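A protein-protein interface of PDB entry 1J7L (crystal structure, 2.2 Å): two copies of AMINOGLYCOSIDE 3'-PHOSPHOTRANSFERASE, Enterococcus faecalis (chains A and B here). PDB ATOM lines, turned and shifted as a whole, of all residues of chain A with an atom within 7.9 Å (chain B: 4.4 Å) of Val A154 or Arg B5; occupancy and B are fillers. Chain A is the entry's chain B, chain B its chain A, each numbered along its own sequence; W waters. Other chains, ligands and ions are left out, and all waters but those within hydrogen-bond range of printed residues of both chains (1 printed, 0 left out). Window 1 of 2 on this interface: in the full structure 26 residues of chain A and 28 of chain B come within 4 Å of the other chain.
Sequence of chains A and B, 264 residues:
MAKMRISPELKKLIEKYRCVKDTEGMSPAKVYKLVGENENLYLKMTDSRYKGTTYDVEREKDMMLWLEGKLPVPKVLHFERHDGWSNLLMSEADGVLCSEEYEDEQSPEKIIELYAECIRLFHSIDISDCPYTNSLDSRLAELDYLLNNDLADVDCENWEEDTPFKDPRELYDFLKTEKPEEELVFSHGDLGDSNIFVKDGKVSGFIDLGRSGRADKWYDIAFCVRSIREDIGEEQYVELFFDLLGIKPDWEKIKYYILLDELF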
ATOM      1  N   MET A  26      -3.297  27.072 -31.132  1.00  0.00           N
ATOM      2  CA  MET A  26      -4.754  27.027 -31.096  1.00  0.00           C
ATOM      3  C   MET A  26      -5.326  25.907 -31.968  1.00  0.00           C
ATOM      4  O   MET A  26      -6.482  25.513 -31.807  1.00  0.00           O
ATOM      5  CB  MET A  26      -5.337  28.368 -31.550  1.00  0.00           C
ATOM      6  CG  MET A  26      -6.770  28.597 -31.077  1.00  0.00           C
ATOM      7  SD  MET A  26      -7.616  29.937 -31.938  1.00  0.00           S
ATOM      8  CE  MET A  26      -8.879  29.002 -32.844  1.00  0.00           C
ATOM      9  N   ARG A  49      -2.938  12.968 -40.214  1.00  0.00           N
ATOM     10  CA  ARG A  49      -4.310  12.811 -39.721  1.00  0.00           C
ATOM     11  C   ARG A  49      -5.296  13.885 -40.187  1.00  0.00           C
ATOM     12  O   ARG A  49      -6.500  13.649 -40.238  1.00  0.00           O
ATOM     13  CB  ARG A  49      -4.300  12.763 -38.192  1.00  0.00           C
ATOM     14  CG  ARG A  49      -3.462  11.624 -37.620  1.00  0.00           C
ATOM     15  CD  ARG A  49      -3.216  11.795 -36.129  1.00  0.00           C
ATOM     16  NE  ARG A  49      -2.574  13.072 -35.818  1.00  0.00           N
ATOM     17  CZ  ARG A  49      -2.577  13.635 -34.614  1.00  0.00           C
ATOM     18  NH1 ARG A  49      -1.973  14.800 -34.420  1.00  0.00           N
ATOM     19  NH2 ARG A  49      -3.183  13.032 -33.602  1.00  0.00           N
ATOM     20  N   TYR A  50      -4.781  15.053 -40.551  1.00  0.00           N
ATOM     21  CA  TYR A  50      -5.629  16.157 -40.977  1.00  0.00           C
ATOM     22  C   TYR A  50      -5.694  16.359 -42.474  1.00  0.00           C
ATOM     23  O   TYR A  50      -6.318  17.305 -42.955  1.00  0.00           O
ATOM     24  CB  TYR A  50      -5.191  17.439 -40.277  1.00  0.00           C
ATOM     25  CG  TYR A  50      -5.330  17.323 -38.787  1.00  0.00           C
ATOM     26  CD1 TYR A  50      -4.230  17.033 -37.983  1.00  0.00           C
ATOM     27  CD2 TYR A  50      -6.568  17.458 -38.181  1.00  0.00           C
ATOM     28  CE1 TYR A  50      -4.366  16.878 -36.611  1.00  0.00           C
ATOM     29  CE2 TYR A  50      -6.715  17.306 -36.815  1.00  0.00           C
ATOM     30  CZ  TYR A  50      -5.613  17.016 -36.036  1.00  0.00           C
ATOM     31  OH  TYR A  50      -5.769  16.878 -34.678  1.00  0.00           O
ATOM     32  N   TYR A  55      -7.968  21.842 -41.916  1.00  0.00           N
ATOM     33  CA  TYR A  55      -6.788  22.114 -41.097  1.00  0.00           C
ATOM     34  C   TYR A  55      -5.529  21.927 -41.953  1.00  0.00           C
ATOM     35  O   TYR A  55      -4.486  22.521 -41.684  1.00  0.00           O
ATOM     36  CB  TYR A  55      -6.705  21.144 -39.922  1.00  0.00           C
ATOM     37  CG  TYR A  55      -7.737  21.346 -38.841  1.00  0.00           C
ATOM     38  CD1 TYR A  55      -8.784  20.444 -38.683  1.00  0.00           C
ATOM     39  CD2 TYR A  55      -7.635  22.405 -37.940  1.00  0.00           C
ATOM     40  CE1 TYR A  55      -9.694  20.582 -37.657  1.00  0.00           C
ATOM     41  CE2 TYR A  55      -8.543  22.553 -36.906  1.00  0.00           C
ATOM     42  CZ  TYR A  55      -9.568  21.632 -36.771  1.00  0.00           C
ATOM     43  OH  TYR A  55     -10.448  21.722 -35.725  1.00  0.00           O
ATOM     44  N   LEU A 146     -13.757  14.060 -38.120  1.00  0.00           N
ATOM     45  CA  LEU A 146     -12.943  14.493 -36.990  1.00  0.00           C
ATOM     46  C   LEU A 146     -13.424  13.835 -35.703  1.00  0.00           C
ATOM     47  O   LEU A 146     -12.621  13.350 -34.910  1.00  0.00           O
ATOM     48  CB  LEU A 146     -12.970  16.021 -36.844  1.00  0.00           C
ATOM     49  CG  LEU A 146     -12.346  16.812 -37.999  1.00  0.00           C
ATOM     50  CD1 LEU A 146     -12.539  18.308 -37.772  1.00  0.00           C
ATOM     51  CD2 LEU A 146     -10.872  16.468 -38.141  1.00  0.00           C
ATOM     52  N   ASN A 149     -12.669  10.070 -35.504  1.00  0.00           N
ATOM     53  CA  ASN A 149     -11.266   9.767 -35.251  1.00  0.00           C
ATOM     54  C   ASN A 149     -10.695  10.515 -34.054  1.00  0.00           C
ATOM     55  O   ASN A 149      -9.484  10.534 -33.854  1.00  0.00           O
ATOM     56  CB  ASN A 149     -10.439  10.045 -36.506  1.00  0.00           C
ATOM     57  CG  ASN A 149     -10.831   9.148 -37.663  1.00  0.00           C
ATOM     58  OD1 ASN A 149     -10.275   8.065 -37.835  1.00  0.00           O
ATOM     59  ND2 ASN A 149     -11.816   9.577 -38.442  1.00  0.00           N
ATOM     60  N   ASP A 150     -11.581  11.127 -33.270  1.00  0.00           N
ATOM     61  CA  ASP A 150     -11.204  11.884 -32.076  1.00  0.00           C
ATOM     62  C   ASP A 150     -10.201  12.997 -32.378  1.00  0.00           C
ATOM     63  O   ASP A 150      -9.280  13.255 -31.599  1.00  0.00           O
ATOM     64  CB  ASP A 150     -10.658  10.940 -30.998  1.00  0.00           C
ATOM     65  CG  ASP A 150     -10.517  11.609 -29.646  1.00  0.00           C
ATOM     66  OD1 ASP A 150     -11.183  12.635 -29.398  1.00  0.00           O
ATOM     67  OD2 ASP A 150      -9.724  11.110 -28.828  1.00  0.00           O
ATOM     68  N   LEU A 151     -10.412  13.670 -33.504  1.00  0.00           N
ATOM     69  CA  LEU A 151      -9.551  14.761 -33.934  1.00  0.00           C
ATOM     70  C   LEU A 151     -10.231  16.117 -33.777  1.00  0.00           C
ATOM     71  O   LEU A 151      -9.630  17.147 -34.079  1.00  0.00           O
ATOM     72  CB  LEU A 151      -9.128  14.560 -35.393  1.00  0.00           C
ATOM     73  CG  LEU A 151      -8.401  13.252 -35.704  1.00  0.00           C
ATOM     74  CD1 LEU A 151      -8.161  13.139 -37.201  1.00  0.00           C
ATOM     75  CD2 LEU A 151      -7.094  13.175 -34.920  1.00  0.00           C
ATOM     76  N   ALA A 152     -11.490  16.117 -33.338  1.00  0.00           N
ATOM     77  CA  ALA A 152     -12.236  17.364 -33.139  1.00  0.00           C
ATOM     78  C   ALA A 152     -11.748  18.080 -31.880  1.00  0.00           C
ATOM     79  O   ALA A 152     -11.319  17.428 -30.924  1.00  0.00           O
ATOM     80  CB  ALA A 152     -13.725  17.093 -33.057  1.00  0.00           C
ATOM     81  N   ASP A 153     -11.863  19.410 -31.882  1.00  0.00           N
ATOM     82  CA  ASP A 153     -11.410  20.279 -30.788  1.00  0.00           C
ATOM     83  C   ASP A 153     -11.527  19.736 -29.373  1.00  0.00           C
ATOM     84  O   ASP A 153     -12.593  19.279 -28.940  1.00  0.00           O
ATOM     85  CB  ASP A 153     -12.074  21.659 -30.863  1.00  0.00           C
ATOM     86  CG  ASP A 153     -11.435  22.674 -29.915  1.00  0.00           C
ATOM     87  OD1 ASP A 153     -11.651  22.574 -28.690  1.00  0.00           O
ATOM     88  OD2 ASP A 153     -10.717  23.580 -30.396  1.00  0.00           O
ATOM     89  N   VAL A 154     -10.411  19.863 -28.654  1.00  0.00           N
ATOM     90  CA  VAL A 154     -10.264  19.414 -27.276  1.00  0.00           C
ATOM     91  C   VAL A 154     -11.325  19.985 -26.338  1.00  0.00           C
ATOM     92  O   VAL A 154     -11.337  21.187 -26.032  1.00  0.00           O
ATOM     93  N   ASP A 155     -12.232  19.109 -25.914  1.00  0.00           N
ATOM     94  CA  ASP A 155     -13.310  19.487 -25.013  1.00  0.00           C
ATOM     95  C   ASP A 155     -12.733  19.989 -23.687  1.00  0.00           C
ATOM     96  O   ASP A 155     -11.942  19.303 -23.052  1.00  0.00           O
ATOM     97  CB  ASP A 155     -14.230  18.284 -24.771  1.00  0.00           C
ATOM     98  N   CYS A 156     -13.069  21.220 -23.323  1.00  0.00           N
ATOM     99  CA  CYS A 156     -12.607  21.828 -22.071  1.00  0.00           C
ATOM    100  C   CYS A 156     -13.853  22.477 -21.494  1.00  0.00           C
ATOM    101  O   CYS A 156     -14.345  22.072 -20.439  1.00  0.00           O
ATOM    102  CB  CYS A 156     -11.495  22.856 -22.357  1.00  0.00           C
ATOM    103  SG  CYS A 156     -10.972  24.044 -21.064  1.00  0.00           S
ATOM    104  N   GLU A 157     -14.407  23.430 -22.237  1.00  0.00           N
ATOM    105  CA  GLU A 157     -15.626  24.105 -21.818  1.00  0.00           C
ATOM    106  C   GLU A 157     -16.808  23.161 -22.040  1.00  0.00           C
ATOM    107  O   GLU A 157     -17.811  23.234 -21.331  1.00  0.00           O
ATOM    108  CB  GLU A 157     -15.828  25.404 -22.603  1.00  0.00           C
ATOM    109  CG  GLU A 157     -14.861  26.518 -22.221  1.00  0.00           C
ATOM    110  N   ASN A 158     -16.651  22.243 -22.994  1.00  0.00           N
ATOM    111  CA  ASN A 158     -17.687  21.263 -23.326  1.00  0.00           C
ATOM    112  C   ASN A 158     -17.952  20.308 -22.166  1.00  0.00           C
ATOM    113  O   ASN A 158     -18.932  19.562 -22.176  1.00  0.00           O
ATOM    114  CB  ASN A 158     -17.276  20.455 -24.559  1.00  0.00           C
ATOM    115  CG  ASN A 158     -16.801  21.332 -25.701  1.00  0.00           C
ATOM    116  OD1 ASN A 158     -15.942  20.931 -26.484  1.00  0.00           O
ATOM    117  ND2 ASN A 158     -17.356  22.537 -25.800  1.00  0.00           N
ATOM    118  N   TRP A 159     -17.052  20.319 -21.187  1.00  0.00           N
ATOM    119  CA  TRP A 159     -17.165  19.474 -20.004  1.00  0.00           C
ATOM    120  C   TRP A 159     -17.974  20.140 -18.896  1.00  0.00           C
ATOM    121  O   TRP A 159     -18.447  19.467 -17.978  1.00  0.00           O
ATOM    122  CB  TRP A 159     -15.776  19.131 -19.465  1.00  0.00           C
ATOM    123  CG  TRP A 159     -14.966  18.284 -20.379  1.00  0.00           C
ATOM    124  CD1 TRP A 159     -15.431  17.434 -21.338  1.00  0.00           C
ATOM    125  CD2 TRP A 159     -13.541  18.172 -20.399  1.00  0.00           C
ATOM    126  NE1 TRP A 159     -14.383  16.792 -21.951  1.00  0.00           N
ATOM    127  CE2 TRP A 159     -13.210  17.226 -21.392  1.00  0.00           C
ATOM    128  CE3 TRP A 159     -12.509  18.779 -19.672  1.00  0.00           C
ATOM    129  CZ2 TRP A 159     -11.889  16.869 -21.678  1.00  0.00           C
ATOM    130  CZ3 TRP A 159     -11.195  18.425 -19.957  1.00  0.00           C
ATOM    131  CH2 TRP A 159     -10.899  17.478 -20.953  1.00  0.00           C
ATOM    132  N   PRO A 168     -20.353  16.089 -28.003  1.00  0.00           N
ATOM    133  CA  PRO A 168     -20.062  16.507 -29.377  1.00  0.00           C
ATOM    134  C   PRO A 168     -21.069  16.000 -30.406  1.00  0.00           C
ATOM    135  O   PRO A 168     -21.486  16.753 -31.287  1.00  0.00           O
ATOM    136  CB  PRO A 168     -18.678  15.917 -29.616  1.00  0.00           C
ATOM    137  CG  PRO A 168     -18.042  16.054 -28.283  1.00  0.00           C
ATOM    138  CD  PRO A 168     -19.133  15.570 -27.355  1.00  0.00           C
ATOM    139  N   GLU A 262     -17.536  25.579 -32.539  1.00  0.00           N
ATOM    140  CA  GLU A 262     -17.263  25.032 -31.211  1.00  0.00           C
ATOM    141  C   GLU A 262     -16.396  23.771 -31.260  1.00  0.00           C
ATOM    142  O   GLU A 262     -15.423  23.654 -30.513  1.00  0.00           O
ATOM    143  CB  GLU A 262     -18.572  24.712 -30.483  1.00  0.00           C
ATOM    144  CG  GLU A 262     -19.496  25.905 -30.298  1.00  0.00           C
ATOM    145  CD  GLU A 262     -19.684  26.302 -28.844  1.00  0.00           C
ATOM    146  OE1 GLU A 262     -19.828  25.403 -27.987  1.00  0.00           O
ATOM    147  OE2 GLU A 262     -19.705  27.518 -28.563  1.00  0.00           O
ATOM    148  N   LEU A 263     -16.733  22.848 -32.160  1.00  0.00           N
ATOM    149  CA  LEU A 263     -15.991  21.597 -32.284  1.00  0.00           C
ATOM    150  C   LEU A 263     -14.714  21.659 -33.118  1.00  0.00           C
ATOM    151  O   LEU A 263     -14.029  20.651 -33.284  1.00  0.00           O
ATOM    152  CB  LEU A 263     -16.905  20.484 -32.800  1.00  0.00           C
ATOM    153  CG  LEU A 263     -18.075  20.135 -31.873  1.00  0.00           C
ATOM    154  CD1 LEU A 263     -18.797  18.906 -32.399  1.00  0.00           C
ATOM    155  CD2 LEU A 263     -17.570  19.887 -30.461  1.00  0.00           C
ATOM    156  N   PHE A 264     -14.400  22.832 -33.654  1.00  0.00           N
ATOM    157  CA  PHE A 264     -13.191  22.997 -34.452  1.00  0.00           C
ATOM    158  C   PHE A 264     -12.100  23.729 -33.681  1.00  0.00           C
ATOM    159  O   PHE A 264     -10.921  23.620 -34.078  1.00  0.00           O
ATOM    160  CB  PHE A 264     -13.502  23.741 -35.747  1.00  0.00           C
ATOM    161  CG  PHE A 264     -14.304  22.938 -36.720  1.00  0.00           C
ATOM    162  CD1 PHE A 264     -15.695  23.019 -36.729  1.00  0.00           C
ATOM    163  CD2 PHE A 264     -13.672  22.090 -37.624  1.00  0.00           C
ATOM    164  CE1 PHE A 264     -16.446  22.265 -37.626  1.00  0.00           C
ATOM    165  CE2 PHE A 264     -14.409  21.329 -38.526  1.00  0.00           C
ATOM    166  CZ  PHE A 264     -15.805  21.418 -38.527  1.00  0.00           C
ATOM    167  OXT PHE A 264     -12.432  24.415 -32.694  1.00  0.00           O
ATOM    168  N   MET B   4     -16.781  10.633 -25.646  1.00  0.00           N
ATOM    169  CA  MET B   4     -16.137  11.672 -24.852  1.00  0.00           C
ATOM    170  C   MET B   4     -14.729  11.192 -24.518  1.00  0.00           C
ATOM    171  O   MET B   4     -14.445   9.992 -24.572  1.00  0.00           O
ATOM    172  CB  MET B   4     -16.907  11.878 -23.548  1.00  0.00           C
ATOM    173  CG  MET B   4     -18.310  12.421 -23.717  1.00  0.00           C
ATOM    174  SD  MET B   4     -18.309  14.203 -23.808  1.00  0.00           S
ATOM    175  CE  MET B   4     -18.788  14.603 -22.126  1.00  0.00           C
ATOM    176  N   ARG B   5     -13.849  12.125 -24.175  1.00  0.00           N
ATOM    177  CA  ARG B   5     -12.480  11.767 -23.814  1.00  0.00           C
ATOM    178  C   ARG B   5     -12.383  11.447 -22.328  1.00  0.00           C
ATOM    179  O   ARG B   5     -11.436  10.796 -21.879  1.00  0.00           O
ATOM    180  CB  ARG B   5     -11.516  12.884 -24.184  1.00  0.00           C
ATOM    181  CG  ARG B   5     -11.373  13.073 -25.672  1.00  0.00           C
ATOM    182  CD  ARG B   5     -10.359  14.146 -25.966  1.00  0.00           C
ATOM    183  NE  ARG B   5     -10.149  14.303 -27.398  1.00  0.00           N
ATOM    184  CZ  ARG B   5      -9.398  15.256 -27.935  1.00  0.00           C
ATOM    185  NH1 ARG B   5      -8.791  16.135 -27.152  1.00  0.00           N
ATOM    186  NH2 ARG B   5      -9.232  15.309 -29.248  1.00  0.00           N
ATOM    187  N   ILE B   6     -13.356  11.931 -21.565  1.00  0.00           N
ATOM    188  CA  ILE B   6     -13.401  11.673 -20.137  1.00  0.00           C
ATOM    189  C   ILE B   6     -14.673  10.894 -19.838  1.00  0.00           C
ATOM    190  O   ILE B   6     -15.637  10.955 -20.598  1.00  0.00           O
ATOM    191  CB  ILE B   6     -13.367  12.970 -19.313  1.00  0.00           C
ATOM    192  CG1 ILE B   6     -14.551  13.872 -19.677  1.00  0.00           C
ATOM    193  CG2 ILE B   6     -12.035  13.687 -19.530  1.00  0.00           C
ATOM    194  CD1 ILE B   6     -14.774  15.006 -18.700  1.00  0.00           C
ATOM    195  N   MET B  45      -4.122  15.040 -19.405  1.00  0.00           N
ATOM    196  CA  MET B  45      -4.554  13.945 -20.267  1.00  0.00           C
ATOM    197  C   MET B  45      -3.571  13.624 -21.377  1.00  0.00           C
ATOM    198  O   MET B  45      -3.013  14.533 -21.992  1.00  0.00           O
ATOM    199  CB  MET B  45      -5.890  14.314 -20.920  1.00  0.00           C
ATOM    200  CG  MET B  45      -7.032  14.603 -19.943  1.00  0.00           C
ATOM    201  SD  MET B  45      -8.476  15.260 -20.808  1.00  0.00           S
ATOM    202  CE  MET B  45      -8.977  13.839 -21.740  1.00  0.00           C
ATOM    203  N   HIS B  82      -9.764   6.082 -20.546  1.00  0.00           N
ATOM    204  CA  HIS B  82     -11.048   6.227 -21.216  1.00  0.00           C
ATOM    205  C   HIS B  82     -10.817   6.446 -22.694  1.00  0.00           C
ATOM    206  O   HIS B  82     -10.194   7.434 -23.089  1.00  0.00           O
ATOM    207  CB  HIS B  82     -11.834   7.402 -20.626  1.00  0.00           C
ATOM    208  CG  HIS B  82     -13.262   7.446 -21.067  1.00  0.00           C
ATOM    209  ND1 HIS B  82     -13.700   8.244 -22.100  1.00  0.00           N
ATOM    210  CD2 HIS B  82     -14.351   6.770 -20.626  1.00  0.00           C
ATOM    211  CE1 HIS B  82     -14.996   8.060 -22.276  1.00  0.00           C
ATOM    212  NE2 HIS B  82     -15.415   7.172 -21.395  1.00  0.00           N
ATOM    213  N   TRP B  85      -7.456   7.416 -23.754  1.00  0.00           N
ATOM    214  CA  TRP B  85      -6.913   8.510 -22.966  1.00  0.00           C
ATOM    215  C   TRP B  85      -6.664   8.133 -21.523  1.00  0.00           C
ATOM    216  O   TRP B  85      -7.458   7.426 -20.906  1.00  0.00           O
ATOM    217  CB  TRP B  85      -7.859   9.713 -22.979  1.00  0.00           C
ATOM    218  CG  TRP B  85      -7.988  10.363 -24.301  1.00  0.00           C
ATOM    219  CD1 TRP B  85      -8.832  10.007 -25.310  1.00  0.00           C
ATOM    220  CD2 TRP B  85      -7.245  11.487 -24.774  1.00  0.00           C
ATOM    221  NE1 TRP B  85      -8.661  10.840 -26.388  1.00  0.00           N
ATOM    222  CE2 TRP B  85      -7.691  11.759 -26.087  1.00  0.00           C
ATOM    223  CE3 TRP B  85      -6.246  12.295 -24.217  1.00  0.00           C
ATOM    224  CZ2 TRP B  85      -7.169  12.807 -26.856  1.00  0.00           C
ATOM    225  CZ3 TRP B  85      -5.726  13.339 -24.982  1.00  0.00           C
ATOM    226  CH2 TRP B  85      -6.192  13.583 -26.288  1.00  0.00           C
ATOM    227  N   ASN B  87      -6.466   9.773 -18.051  1.00  0.00           N
ATOM    228  CA  ASN B  87      -6.899  11.017 -17.431  1.00  0.00           C
ATOM    229  C   ASN B  87      -6.566  11.104 -15.960  1.00  0.00           C
ATOM    230  O   ASN B  87      -7.002  10.269 -15.172  1.00  0.00           O
ATOM    231  CB  ASN B  87      -8.408  11.188 -17.630  1.00  0.00           C
ATOM    232  CG  ASN B  87      -8.810  11.097 -19.083  1.00  0.00           C
ATOM    233  OD1 ASN B  87      -8.064  11.521 -19.972  1.00  0.00           O
ATOM    234  ND2 ASN B  87      -9.978  10.525 -19.341  1.00  0.00           N
HETATM  235  O   HOH W   1     -10.918   8.523 -27.621  1.00  0.00           O
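No position is printed for both chains. Of the 7 pairs that touch across the chains among the printed residues, none has its exchanged pair printed and touching as well.
Printed residues of chain A that touch a printed residue of chain B: Asp A150, Ala A152, Val A154, Trp A159 and Pro A168. Hydrophobic or aromatic side chains of chain A that line the printed part of chain B: Trp A159 and Pro A168. Of the 7 printed residues of chain B, 5 touch a printed residue of chain A. Hydrophobic or aromatic side chains of chain B that line the printed part of chain A: Met B4, Ile B6, Met B45 and Trp B85. Among the printed residues, 7 pairs touch across the chains.
NE of Arg B5 lies within salt-bridge range of OD1 of Asp A150, at 2.8 Å. The guanidinium group (NH2) of Arg B5 sits at hydrogen-bond distance from the backbone carbonyl oxygen (O) of Ala A152, at 3.4 Å. The indole nitrogen of Trp B85 sits at hydrogen-bond distance from the side-chain carboxylate of Asp A150.
ND1 of His B82 lies close to O of Met B4 (3.1 Å). O of Arg B5 sits at hydrogen-bond distance from ND1 of His B82, at 3.4 Å. The backbone carbonyl oxygen of Arg B5 sits at hydrogen-bond distance from the side-chain amide nitrogen of Asn B87 (2.9 Å). O of Leu A146 sits at hydrogen-bond distance from N of Ala A152, at 3.4 Å.
Arg B5 touches Val A154 (NH1 to CA, 3.6 Å). Ile B6 touches Trp A159. Met B45 touches Trp A159 (SD to CH2, 3.3 Å). CD of Pro A168 touches SD of Met B4, 3.9 Å away.
Of the printed residues of chain B, Ala A152 touches Arg B5 (3.4 Å). Printed residues of chain A within 4 Å of Trp B85: Asp A150. Printed residues of chain B within 4 Å of Pro A168: Met B4. Phe A264 touches none of the printed residues of chain B. The nearest printed residue of chain B that does not touch Val A154 is Trp B85 (7.2 Å). The nearest printed residue of chain A that does not touch Met B4 is Trp A159 (4.5 Å).
Water W1 bridges OD2 of Asp A150 and NE1 of Trp B85.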
